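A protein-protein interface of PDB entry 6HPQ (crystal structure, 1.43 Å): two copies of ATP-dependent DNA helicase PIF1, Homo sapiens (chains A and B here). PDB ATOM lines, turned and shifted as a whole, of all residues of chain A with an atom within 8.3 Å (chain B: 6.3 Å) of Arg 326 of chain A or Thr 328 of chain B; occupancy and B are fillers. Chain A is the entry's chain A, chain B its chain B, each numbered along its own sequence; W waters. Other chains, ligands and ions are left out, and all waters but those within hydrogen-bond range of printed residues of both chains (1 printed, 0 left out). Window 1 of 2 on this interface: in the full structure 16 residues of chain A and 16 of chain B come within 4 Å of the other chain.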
ATOM      1  N   MET A 251       2.921  25.446  23.047  1.00  0.00           N
ATOM      2  CA  MET A 251       2.489  24.174  22.416  1.00  0.00           C
ATOM      3  C   MET A 251       2.885  24.255  20.935  1.00  0.00           C
ATOM      4  O   MET A 251       2.391  25.191  20.256  1.00  0.00           O
ATOM      5  CB  MET A 251       0.972  23.968  22.601  1.00  0.00           C
ATOM      6  CG  MET A 251       0.379  22.688  22.015  1.00  0.00           C
ATOM      7  SD  MET A 251       1.259  21.171  22.402  1.00  0.00           S
ATOM      8  CE  MET A 251       0.956  20.100  20.977  1.00  0.00           C
ATOM      9  N   LEU A 261      11.366  26.455  13.561  1.00  0.00           N
ATOM     10  CA  LEU A 261      10.307  27.388  13.991  1.00  0.00           C
ATOM     11  C   LEU A 261      10.898  28.608  14.728  1.00  0.00           C
ATOM     12  O   LEU A 261      10.448  29.725  14.442  1.00  0.00           O
ATOM     13  CB  LEU A 261       9.315  26.652  14.874  1.00  0.00           C
ATOM     14  CG  LEU A 261       8.177  27.556  15.297  1.00  0.00           C
ATOM     15  CD1 LEU A 261       6.872  26.958  14.870  1.00  0.00           C
ATOM     16  CD2 LEU A 261       8.238  27.811  16.776  1.00  0.00           C
ATOM     17  N   CYS A 265      10.038  32.563  14.555  1.00  0.00           N
ATOM     18  CA  CYS A 265       9.097  32.961  15.632  1.00  0.00           C
ATOM     19  C   CYS A 265       9.801  33.779  16.732  1.00  0.00           C
ATOM     20  O   CYS A 265      10.891  33.425  17.201  1.00  0.00           O
ATOM     21  CB  CYS A 265       8.449  31.669  16.110  1.00  0.00           C
ATOM     22  SG  CYS A 265       7.370  31.929  17.514  1.00  0.00           S
ATOM     23  N   PRO A 266       9.239  34.928  17.180  1.00  0.00           N
ATOM     24  CA  PRO A 266       9.910  35.801  18.156  1.00  0.00           C
ATOM     25  C   PRO A 266       9.650  35.451  19.626  1.00  0.00           C
ATOM     26  O   PRO A 266      10.001  36.207  20.521  1.00  0.00           O
ATOM     27  CB  PRO A 266       9.290  37.190  17.838  1.00  0.00           C
ATOM     28  CG  PRO A 266       7.862  36.858  17.382  1.00  0.00           C
ATOM     29  CD  PRO A 266       7.968  35.500  16.700  1.00  0.00           C
ATOM     30  N   VAL A 267       8.984  34.334  19.890  1.00  0.00           N
ATOM     31  CA  VAL A 267       8.711  33.912  21.294  1.00  0.00           C
ATOM     32  C   VAL A 267       9.292  32.522  21.521  1.00  0.00           C
ATOM     33  O   VAL A 267       9.545  31.778  20.560  1.00  0.00           O
ATOM     34  CB  VAL A 267       7.209  33.953  21.652  1.00  0.00           C
ATOM     35  CG1 VAL A 267       6.601  35.334  21.465  1.00  0.00           C
ATOM     36  CG2 VAL A 267       6.399  32.976  20.825  1.00  0.00           C
ATOM     37  N   VAL A 282       5.180  41.180  20.697  1.00  0.00           N
ATOM     38  CA  VAL A 282       5.724  40.786  19.382  1.00  0.00           C
ATOM     39  C   VAL A 282       4.616  40.361  18.425  1.00  0.00           C
ATOM     40  O   VAL A 282       4.933  39.607  17.503  1.00  0.00           O
ATOM     41  CB  VAL A 282       6.840  39.752  19.533  1.00  0.00           C
ATOM     42  CG1 VAL A 282       8.051  40.431  20.149  1.00  0.00           C
ATOM     43  CG2 VAL A 282       6.431  38.524  20.319  1.00  0.00           C
ATOM     44  N   LYS A 283       3.394  40.876  18.612  1.00  0.00           N
ATOM     45  CA  LYS A 283       2.322  40.753  17.603  1.00  0.00           C
ATOM     46  C   LYS A 283       1.527  42.058  17.589  1.00  0.00           C
ATOM     47  O   LYS A 283       1.386  42.748  18.631  1.00  0.00           O
ATOM     48  CB  LYS A 283       1.507  39.467  17.818  1.00  0.00           C
ATOM     49  CG  LYS A 283       1.206  38.738  16.501  1.00  0.00           C
ATOM     50  CD  LYS A 283       0.913  37.284  16.667  1.00  0.00           C
ATOM     51  CE  LYS A 283       1.465  36.394  15.582  1.00  0.00           C
ATOM     52  NZ  LYS A 283       0.568  36.345  14.418  1.00  0.00           N
ATOM     53  N   HIS A 323      -3.130  37.859  26.066  1.00  0.00           N
ATOM     54  CA  HIS A 323      -3.748  36.546  25.805  1.00  0.00           C
ATOM     55  C   HIS A 323      -2.870  35.769  24.821  1.00  0.00           C
ATOM     56  O   HIS A 323      -1.967  36.365  24.197  1.00  0.00           O
ATOM     57  CB  HIS A 323      -5.172  36.738  25.280  1.00  0.00           C
ATOM     58  CG  HIS A 323      -6.123  37.310  26.280  1.00  0.00           C
ATOM     59  ND1 HIS A 323      -6.368  38.679  26.417  1.00  0.00           N
ATOM     60  CD2 HIS A 323      -6.906  36.695  27.188  1.00  0.00           C
ATOM     61  CE1 HIS A 323      -7.286  38.876  27.346  1.00  0.00           C
ATOM     62  NE2 HIS A 323      -7.635  37.669  27.851  1.00  0.00           N
ATOM     63  N   ALA A 324      -3.076  34.465  24.733  1.00  0.00           N
ATOM     64  CA  ALA A 324      -2.380  33.579  23.795  1.00  0.00           C
ATOM     65  C   ALA A 324      -2.492  34.098  22.354  1.00  0.00           C
ATOM     66  O   ALA A 324      -3.504  34.641  21.920  1.00  0.00           O
ATOM     67  CB  ALA A 324      -2.973  32.197  23.900  1.00  0.00           C
ATOM     68  N   ASP A 325      -1.489  33.765  21.581  1.00  0.00           N
ATOM     69  CA  ASP A 325      -1.515  33.964  20.133  1.00  0.00           C
ATOM     70  C   ASP A 325      -0.846  32.770  19.464  1.00  0.00           C
ATOM     71  O   ASP A 325      -0.493  31.793  20.126  1.00  0.00           O
ATOM     72  CB  ASP A 325      -0.909  35.297  19.735  1.00  0.00           C
ATOM     73  CG  ASP A 325      -1.652  35.942  18.581  1.00  0.00           C
ATOM     74  OD1 ASP A 325      -1.934  35.251  17.587  1.00  0.00           O
ATOM     75  OD2 ASP A 325      -1.932  37.138  18.683  1.00  0.00           O
ATOM     76  N   ARG A 326      -0.688  32.865  18.150  1.00  0.00           N
ATOM     77  CA  ARG A 326      -0.199  31.715  17.389  1.00  0.00           C
ATOM     78  C   ARG A 326       0.660  32.221  16.245  1.00  0.00           C
ATOM     79  O   ARG A 326       0.365  33.311  15.707  1.00  0.00           O
ATOM     80  CB  ARG A 326      -1.432  30.894  16.998  1.00  0.00           C
ATOM     81  CG  ARG A 326      -1.052  29.545  16.442  1.00  0.00           C
ATOM     82  CD  ARG A 326      -1.091  29.742  14.967  1.00  0.00           C
ATOM     83  NE  ARG A 326      -2.449  29.486  14.521  1.00  0.00           N
ATOM     84  CZ  ARG A 326      -2.952  29.916  13.377  1.00  0.00           C
ATOM     85  NH1 ARG A 326      -4.199  29.599  13.055  1.00  0.00           N
ATOM     86  NH2 ARG A 326      -2.210  30.671  12.579  1.00  0.00           N
ATOM     87  N   TRP A 327       1.689  31.453  15.925  1.00  0.00           N
ATOM     88  CA  TRP A 327       2.593  31.664  14.757  1.00  0.00           C
ATOM     89  C   TRP A 327       2.546  30.423  13.883  1.00  0.00           C
ATOM     90  O   TRP A 327       2.566  29.316  14.408  1.00  0.00           O
ATOM     91  CB  TRP A 327       4.024  31.969  15.216  1.00  0.00           C
ATOM     92  CG  TRP A 327       4.143  33.275  15.936  1.00  0.00           C
ATOM     93  CD1 TRP A 327       4.571  34.478  15.452  1.00  0.00           C
ATOM     94  CD2 TRP A 327       3.750  33.513  17.297  1.00  0.00           C
ATOM     95  NE1 TRP A 327       4.489  35.438  16.435  1.00  0.00           N
ATOM     96  CE2 TRP A 327       3.976  34.869  17.569  1.00  0.00           C
ATOM     97  CE3 TRP A 327       3.224  32.683  18.306  1.00  0.00           C
ATOM     98  CZ2 TRP A 327       3.711  35.414  18.819  1.00  0.00           C
ATOM     99  CZ3 TRP A 327       2.931  33.232  19.523  1.00  0.00           C
ATOM    100  CH2 TRP A 327       3.166  34.585  19.770  1.00  0.00           C
ATOM    101  N   THR A 328       2.439  30.613  12.578  1.00  0.00           N
ATOM    102  CA  THR A 328       2.555  29.485  11.634  1.00  0.00           C
ATOM    103  C   THR A 328       3.710  29.790  10.722  1.00  0.00           C
ATOM    104  O   THR A 328       3.739  30.864  10.143  1.00  0.00           O
ATOM    105  CB  THR A 328       1.316  29.229  10.795  1.00  0.00           C
ATOM    106  OG1 THR A 328       1.149  30.409  10.020  1.00  0.00           O
ATOM    107  CG2 THR A 328       0.140  28.922  11.679  1.00  0.00           C
ATOM    108  N   VAL A 329       4.618  28.843  10.641  1.00  0.00           N
ATOM    109  CA  VAL A 329       5.901  29.010   9.934  1.00  0.00           C
ATOM    110  C   VAL A 329       5.872  28.035   8.762  1.00  0.00           C
ATOM    111  O   VAL A 329       5.510  26.855   9.005  1.00  0.00           O
ATOM    112  CB  VAL A 329       7.048  28.735  10.918  1.00  0.00           C
ATOM    113  CG1 VAL A 329       8.354  28.452  10.196  1.00  0.00           C
ATOM    114  CG2 VAL A 329       7.200  29.902  11.895  1.00  0.00           C
ATOM    115  N   LEU A 336       4.067  23.069   7.099  1.00  0.00           N
ATOM    116  CA  LEU A 336       3.707  24.158   8.040  1.00  0.00           C
ATOM    117  C   LEU A 336       3.872  23.649   9.482  1.00  0.00           C
ATOM    118  O   LEU A 336       3.493  22.515   9.808  1.00  0.00           O
ATOM    119  CB  LEU A 336       2.275  24.616   7.808  1.00  0.00           C
ATOM    120  CG  LEU A 336       1.919  25.113   6.427  1.00  0.00           C
ATOM    121  CD1 LEU A 336       0.458  25.505   6.367  1.00  0.00           C
ATOM    122  CD2 LEU A 336       2.785  26.290   6.050  1.00  0.00           C
ATOM    123  N   LEU A 337       4.409  24.519  10.308  1.00  0.00           N
ATOM    124  CA  LEU A 337       4.664  24.326  11.756  1.00  0.00           C
ATOM    125  C   LEU A 337       3.917  25.429  12.510  1.00  0.00           C
ATOM    126  O   LEU A 337       3.938  26.609  12.045  1.00  0.00           O
ATOM    127  CB  LEU A 337       6.171  24.483  11.999  1.00  0.00           C
ATOM    128  CG  LEU A 337       7.119  23.691  11.096  1.00  0.00           C
ATOM    129  CD1 LEU A 337       8.565  23.977  11.497  1.00  0.00           C
ATOM    130  CD2 LEU A 337       6.820  22.208  11.189  1.00  0.00           C
ATOM    131  N   SER A 338       3.380  25.137  13.688  1.00  0.00           N
ATOM    132  CA  SER A 338       2.763  26.202  14.506  1.00  0.00           C
ATOM    133  C   SER A 338       3.329  26.197  15.923  1.00  0.00           C
ATOM    134  O   SER A 338       3.813  25.131  16.420  1.00  0.00           O
ATOM    135  CB  SER A 338       1.252  26.132  14.528  1.00  0.00           C
ATOM    136  OG  SER A 338       0.824  24.938  15.152  1.00  0.00           O
ATOM    137  N   ARG A 339       3.200  27.363  16.547  1.00  0.00           N
ATOM    138  CA  ARG A 339       3.454  27.534  17.985  1.00  0.00           C
ATOM    139  C   ARG A 339       2.342  28.411  18.565  1.00  0.00           C
ATOM    140  O   ARG A 339       2.027  29.495  18.008  1.00  0.00           O
ATOM    141  CB  ARG A 339       4.799  28.210  18.222  1.00  0.00           C
ATOM    142  CG  ARG A 339       5.014  28.647  19.671  1.00  0.00           C
ATOM    143  CD  ARG A 339       6.442  28.975  20.010  1.00  0.00           C
ATOM    144  NE  ARG A 339       7.313  27.795  19.974  1.00  0.00           N
ATOM    145  CZ  ARG A 339       8.647  27.851  19.961  1.00  0.00           C
ATOM    146  NH1 ARG A 339       9.328  26.722  19.886  1.00  0.00           N
ATOM    147  NH2 ARG A 339       9.277  29.021  19.949  1.00  0.00           N
ATOM    148  N   GLN A 340       1.810  27.962  19.677  1.00  0.00           N
ATOM    149  CA  GLN A 340       0.891  28.746  20.545  1.00  0.00           C
ATOM    150  C   GLN A 340       1.651  29.195  21.784  1.00  0.00           C
ATOM    151  O   GLN A 340       2.227  28.357  22.497  1.00  0.00           O
ATOM    152  CB  GLN A 340      -0.256  27.906  21.060  1.00  0.00           C
ATOM    153  CG  GLN A 340      -1.281  27.508  20.017  1.00  0.00           C
ATOM    154  CD  GLN A 340      -2.360  26.761  20.756  1.00  0.00           C
ATOM    155  OE1 GLN A 340      -3.129  27.317  21.567  1.00  0.00           O
ATOM    156  NE2 GLN A 340      -2.330  25.460  20.563  1.00  0.00           N
ATOM    157  N   GLN A 341       1.653  30.491  22.010  1.00  0.00           N
ATOM    158  CA  GLN A 341       2.392  31.108  23.145  1.00  0.00           C
ATOM    159  C   GLN A 341       1.853  32.517  23.346  1.00  0.00           C
ATOM    160  O   GLN A 341       1.227  33.055  22.413  1.00  0.00           O
ATOM    161  CB  GLN A 341       3.894  31.066  22.824  1.00  0.00           C
ATOM    162  CG  GLN A 341       4.850  31.675  23.846  1.00  0.00           C
ATOM    163  CD  GLN A 341       4.835  30.997  25.201  1.00  0.00           C
ATOM    164  OE1 GLN A 341       5.775  30.263  25.618  1.00  0.00           O
ATOM    165  NE2 GLN A 341       3.783  31.240  25.915  1.00  0.00           N
ATOM    166  N   LEU A 342       2.117  33.121  24.502  1.00  0.00           N
ATOM    167  CA  LEU A 342       1.828  34.559  24.672  1.00  0.00           C
ATOM    168  C   LEU A 342       2.788  35.310  23.749  1.00  0.00           C
ATOM    169  O   LEU A 342       3.938  34.963  23.666  1.00  0.00           O
ATOM    170  CB  LEU A 342       2.062  34.987  26.121  1.00  0.00           C
ATOM    171  CG  LEU A 342       1.313  34.222  27.199  1.00  0.00           C
ATOM    172  CD1 LEU A 342       1.452  34.931  28.531  1.00  0.00           C
ATOM    173  CD2 LEU A 342      -0.134  34.011  26.845  1.00  0.00           C
ATOM    174  N   PRO A 343       2.345  36.425  23.132  1.00  0.00           N
ATOM    175  CA  PRO A 343       3.199  37.234  22.272  1.00  0.00           C
ATOM    176  C   PRO A 343       4.075  38.235  23.054  1.00  0.00           C
ATOM    177  O   PRO A 343       4.070  39.417  22.780  1.00  0.00           O
ATOM    178  CB  PRO A 343       2.167  37.945  21.372  1.00  0.00           C
ATOM    179  CG  PRO A 343       1.007  38.145  22.296  1.00  0.00           C
ATOM    180  CD  PRO A 343       0.943  36.865  23.094  1.00  0.00           C
ATOM    181  N   GLY B  63     -10.202  24.744  16.503  1.00  0.00           N
ATOM    182  CA  GLY B  63      -9.775  23.368  16.708  1.00  0.00           C
ATOM    183  C   GLY B  63      -9.669  22.599  15.421  1.00  0.00           C
ATOM    184  O   GLY B  63      -9.609  23.187  14.303  1.00  0.00           O
ATOM    185  N   LEU B 261      -8.927  19.806   3.602  1.00  0.00           N
ATOM    186  CA  LEU B 261      -8.973  21.250   3.879  1.00  0.00           C
ATOM    187  C   LEU B 261     -10.397  21.793   3.680  1.00  0.00           C
ATOM    188  O   LEU B 261     -10.824  22.530   4.550  1.00  0.00           O
ATOM    189  CB  LEU B 261      -7.997  22.008   3.000  1.00  0.00           C
ATOM    190  CG  LEU B 261      -8.020  23.497   3.298  1.00  0.00           C
ATOM    191  CD1 LEU B 261      -6.654  23.962   3.716  1.00  0.00           C
ATOM    192  CD2 LEU B 261      -8.551  24.258   2.121  1.00  0.00           C
ATOM    193  N   GLN B 264     -13.051  21.729   6.504  1.00  0.00           N
ATOM    194  CA  GLN B 264     -12.885  22.666   7.632  1.00  0.00           C
ATOM    195  C   GLN B 264     -12.942  24.106   7.115  1.00  0.00           C
ATOM    196  O   GLN B 264     -13.332  24.995   7.877  1.00  0.00           O
ATOM    197  CB  GLN B 264     -11.623  22.319   8.419  1.00  0.00           C
ATOM    198  CG  GLN B 264     -11.613  20.918   9.051  1.00  0.00           C
ATOM    199  CD  GLN B 264     -10.583  20.846  10.159  1.00  0.00           C
ATOM    200  OE1 GLN B 264     -10.488  21.770  10.959  1.00  0.00           O
ATOM    201  NE2 GLN B 264      -9.769  19.789  10.187  1.00  0.00           N
ATOM    202  N   ARG B 326      -6.711  33.898   5.273  1.00  0.00           N
ATOM    203  CA  ARG B 326      -6.005  32.609   5.306  1.00  0.00           C
ATOM    204  C   ARG B 326      -6.694  31.717   6.320  1.00  0.00           C
ATOM    205  O   ARG B 326      -7.148  32.239   7.356  1.00  0.00           O
ATOM    206  CB  ARG B 326      -4.536  32.883   5.667  1.00  0.00           C
ATOM    207  CG  ARG B 326      -3.774  31.668   6.147  1.00  0.00           C
ATOM    208  CD  ARG B 326      -2.893  31.156   5.041  1.00  0.00           C
ATOM    209  NE  ARG B 326      -1.743  30.415   5.542  1.00  0.00           N
ATOM    210  CZ  ARG B 326      -0.553  30.378   4.956  1.00  0.00           C
ATOM    211  NH1 ARG B 326      -0.350  31.063   3.835  1.00  0.00           N
ATOM    212  NH2 ARG B 326       0.417  29.645   5.493  1.00  0.00           N
ATOM    213  N   TRP B 327      -6.745  30.437   6.008  1.00  0.00           N
ATOM    214  CA  TRP B 327      -7.226  29.350   6.900  1.00  0.00           C
ATOM    215  C   TRP B 327      -6.090  28.356   7.080  1.00  0.00           C
ATOM    216  O   TRP B 327      -5.414  28.020   6.125  1.00  0.00           O
ATOM    217  CB  TRP B 327      -8.471  28.684   6.311  1.00  0.00           C
ATOM    218  CG  TRP B 327      -9.644  29.609   6.295  1.00  0.00           C
ATOM    219  CD1 TRP B 327     -10.701  29.671   7.157  1.00  0.00           C
ATOM    220  CD2 TRP B 327      -9.864  30.633   5.315  1.00  0.00           C
ATOM    221  NE1 TRP B 327     -11.562  30.676   6.768  1.00  0.00           N
ATOM    222  CE2 TRP B 327     -11.062  31.279   5.639  1.00  0.00           C
ATOM    223  CE3 TRP B 327      -9.123  31.059   4.189  1.00  0.00           C
ATOM    224  CZ2 TRP B 327     -11.549  32.335   4.869  1.00  0.00           C
ATOM    225  CZ3 TRP B 327      -9.595  32.105   3.443  1.00  0.00           C
ATOM    226  CH2 TRP B 327     -10.789  32.746   3.795  1.00  0.00           C
ATOM    227  N   THR B 328      -5.880  27.902   8.310  1.00  0.00           N
ATOM    228  CA  THR B 328      -4.912  26.825   8.576  1.00  0.00           C
ATOM    229  C   THR B 328      -5.681  25.722   9.260  1.00  0.00           C
ATOM    230  O   THR B 328      -6.359  26.002  10.233  1.00  0.00           O
ATOM    231  CB  THR B 328      -3.734  27.268   9.431  1.00  0.00           C
ATOM    232  OG1 THR B 328      -4.313  27.650  10.676  1.00  0.00           O
ATOM    233  CG2 THR B 328      -2.969  28.372   8.756  1.00  0.00           C
ATOM    234  N   VAL B 329      -5.600  24.544   8.677  1.00  0.00           N
ATOM    235  CA  VAL B 329      -6.378  23.348   9.063  1.00  0.00           C
ATOM    236  C   VAL B 329      -5.382  22.333   9.634  1.00  0.00           C
ATOM    237  O   VAL B 329      -4.331  22.100   8.989  1.00  0.00           O
ATOM    238  CB  VAL B 329      -7.143  22.809   7.842  1.00  0.00           C
ATOM    239  CG1 VAL B 329      -7.594  21.372   8.046  1.00  0.00           C
ATOM    240  CG2 VAL B 329      -8.323  23.715   7.490  1.00  0.00           C
ATOM    241  N   GLN B 330      -5.684  21.787  10.814  1.00  0.00           N
ATOM    242  CA  GLN B 330      -4.887  20.713  11.473  1.00  0.00           C
ATOM    243  C   GLN B 330      -5.456  19.383  10.983  1.00  0.00           C
ATOM    244  O   GLN B 330      -6.590  19.044  11.298  1.00  0.00           O
ATOM    245  CB  GLN B 330      -4.920  20.904  12.987  1.00  0.00           C
ATOM    246  CG  GLN B 330      -4.081  19.896  13.756  1.00  0.00           C
ATOM    247  CD  GLN B 330      -4.305  20.072  15.242  1.00  0.00           C
ATOM    248  OE1 GLN B 330      -4.652  21.162  15.696  1.00  0.00           O
ATOM    249  NE2 GLN B 330      -4.091  19.012  16.012  1.00  0.00           N
ATOM    250  N   LEU B 336      -0.287  20.379   9.251  1.00  0.00           N
ATOM    251  CA  LEU B 336      -1.029  21.638   9.010  1.00  0.00           C
ATOM    252  C   LEU B 336      -1.107  21.927   7.503  1.00  0.00           C
ATOM    253  O   LEU B 336      -0.104  21.815   6.769  1.00  0.00           O
ATOM    254  CB  LEU B 336      -0.308  22.779   9.710  1.00  0.00           C
ATOM    255  CG  LEU B 336      -0.151  22.650  11.210  1.00  0.00           C
ATOM    256  CD1 LEU B 336       0.612  23.843  11.779  1.00  0.00           C
ATOM    257  CD2 LEU B 336      -1.511  22.493  11.878  1.00  0.00           C
ATOM    258  N   LEU B 337      -2.279  22.362   7.083  1.00  0.00           N
ATOM    259  CA  LEU B 337      -2.602  22.725   5.684  1.00  0.00           C
ATOM    260  C   LEU B 337      -3.103  24.165   5.692  1.00  0.00           C
ATOM    261  O   LEU B 337      -3.870  24.528   6.614  1.00  0.00           O
ATOM    262  CB  LEU B 337      -3.704  21.817   5.141  1.00  0.00           C
ATOM    263  CG  LEU B 337      -3.591  20.323   5.431  1.00  0.00           C
ATOM    264  CD1 LEU B 337      -4.808  19.607   4.845  1.00  0.00           C
ATOM    265  CD2 LEU B 337      -2.278  19.776   4.878  1.00  0.00           C
ATOM    266  N   SER B 338      -2.768  24.943   4.670  1.00  0.00           N
ATOM    267  CA  SER B 338      -3.316  26.307   4.560  1.00  0.00           C
ATOM    268  C   SER B 338      -3.978  26.558   3.205  1.00  0.00           C
ATOM    269  O   SER B 338      -3.630  25.892   2.184  1.00  0.00           O
ATOM    270  CB  SER B 338      -2.273  27.322   4.851  1.00  0.00           C
ATOM    271  OG  SER B 338      -1.299  27.290   3.833  1.00  0.00           O
ATOM    272  N   ARG B 339      -4.912  27.520   3.236  1.00  0.00           N
ATOM    273  CA  ARG B 339      -5.534  28.096   2.035  1.00  0.00           C
ATOM    274  C   ARG B 339      -5.549  29.615   2.186  1.00  0.00           C
ATOM    275  O   ARG B 339      -5.964  30.128   3.247  1.00  0.00           O
ATOM    276  CB  ARG B 339      -6.958  27.590   1.855  1.00  0.00           C
ATOM    277  CG  ARG B 339      -7.754  28.230   0.718  1.00  0.00           C
ATOM    278  CD  ARG B 339      -8.066  27.178  -0.330  1.00  0.00           C
ATOM    279  NE  ARG B 339      -9.359  26.722  -0.100  1.00  0.00           N
ATOM    280  CZ  ARG B 339      -9.866  25.570  -0.498  1.00  0.00           C
ATOM    281  NH1 ARG B 339      -9.178  24.660  -1.174  1.00  0.00           N
ATOM    282  NH2 ARG B 339     -11.103  25.336  -0.162  1.00  0.00           N
HETATM  283  O   HOH W   1       2.467  20.187   9.051  1.00  0.00           O
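OG1 of Thr 328 of chain B lies within hydrogen-bond range of NH1 of Arg 326 of chain A.
N of Val 329 of chain B lies within hydrogen-bond range of O of Leu 337 of chain B. The side-chain amino group of Lys 283 of chain A sits close to the backbone carbonyl oxygen of Arg 326 of chain A, 3.3 Å away. N of Val 329 of chain A sits at hydrogen-bond distance from O of Leu 337 of chain A (2.7 Å). OG of Ser 338 of chain B is in hydrogen-bond range of NH2 of Arg 326 of chain B, 3.4 Å away.
CB of Leu 336 of chain B touches CB of Leu 336 of chain A, at 3.7 Å. C of Leu 337 of chain B touches CD1 of Leu 336 of chain A, 3.9 Å away. Leu 336 of chain A touches Ser 338 of chain B. CD1 of Leu 336 of chain B touches C of Leu 337 of chain A (3.7 Å). CD1 of Leu 336 of chain B touches OG of Ser 338 of chain A, 3.6 Å away.
Of chain B, only Thr 328 (3.1 Å) comes within 4 Å of Arg 326 of chain A. Printed residues of chain B within 4 Å of Leu 337 of chain A: Leu 336 (3.7 Å). Printed residues of chain B within 4 Å of Ser 338 of chain A: Leu 336 (3.6 Å). Leu 342 of chain A touches none of the printed residues of chain B. Of the printed residues of chain A, Leu 337 of chain B touches Leu 336 (3.9 Å). Arg 339 of chain B touches none of the printed residues of chain A. The nearest residue of chain A that does not touch Thr 328 of chain B is Thr 328 of chain A (4.3 Å).
Of the 12 printed residues of chain B, 4 touch a printed residue of chain A. Printed residues of chain B that touch a printed residue of chain A: Thr 328, Leu 336, Leu 337 and Ser 338. Hydrophobic or aromatic side chains of chain A that line the printed part of chain B: Leu 336. Among the printed residues, 6 pairs touch across the chains. Among the printed residues, no Asp or Glu carboxylate lies within 4 Å of a Lys or Arg side-chain nitrogen of the other chain.
Arg 326 of chain A touches Thr 328 of chain B, but with the chains exchanged Thr 328 of chain A does not touch Arg 326 of chain B (4.6 Å). Leu 336 of chain A touches its own counterpart, Leu 336 of chain B. Leu 336 of chain A touches Leu 337 of chain B, and with the chains exchanged Leu 337 of chain A touches Leu 336 of chain B. Leu 336 of chain A touches Ser 338 of chain B, and with the chains exchanged Ser 338 of chain A touches Leu 336 of chain B. Positions printed for both chains: 261, 326, 327, 328, 329, 336, 337, 338 and 339. Of the 6 pairs that touch across the chains among the printed residues, 5 have their exchanged pair printed and touching as well.
Water W1 bridges the backbone carbonyl oxygen of Leu 336 of chain A and the backbone NH of Leu 336 of chain B.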
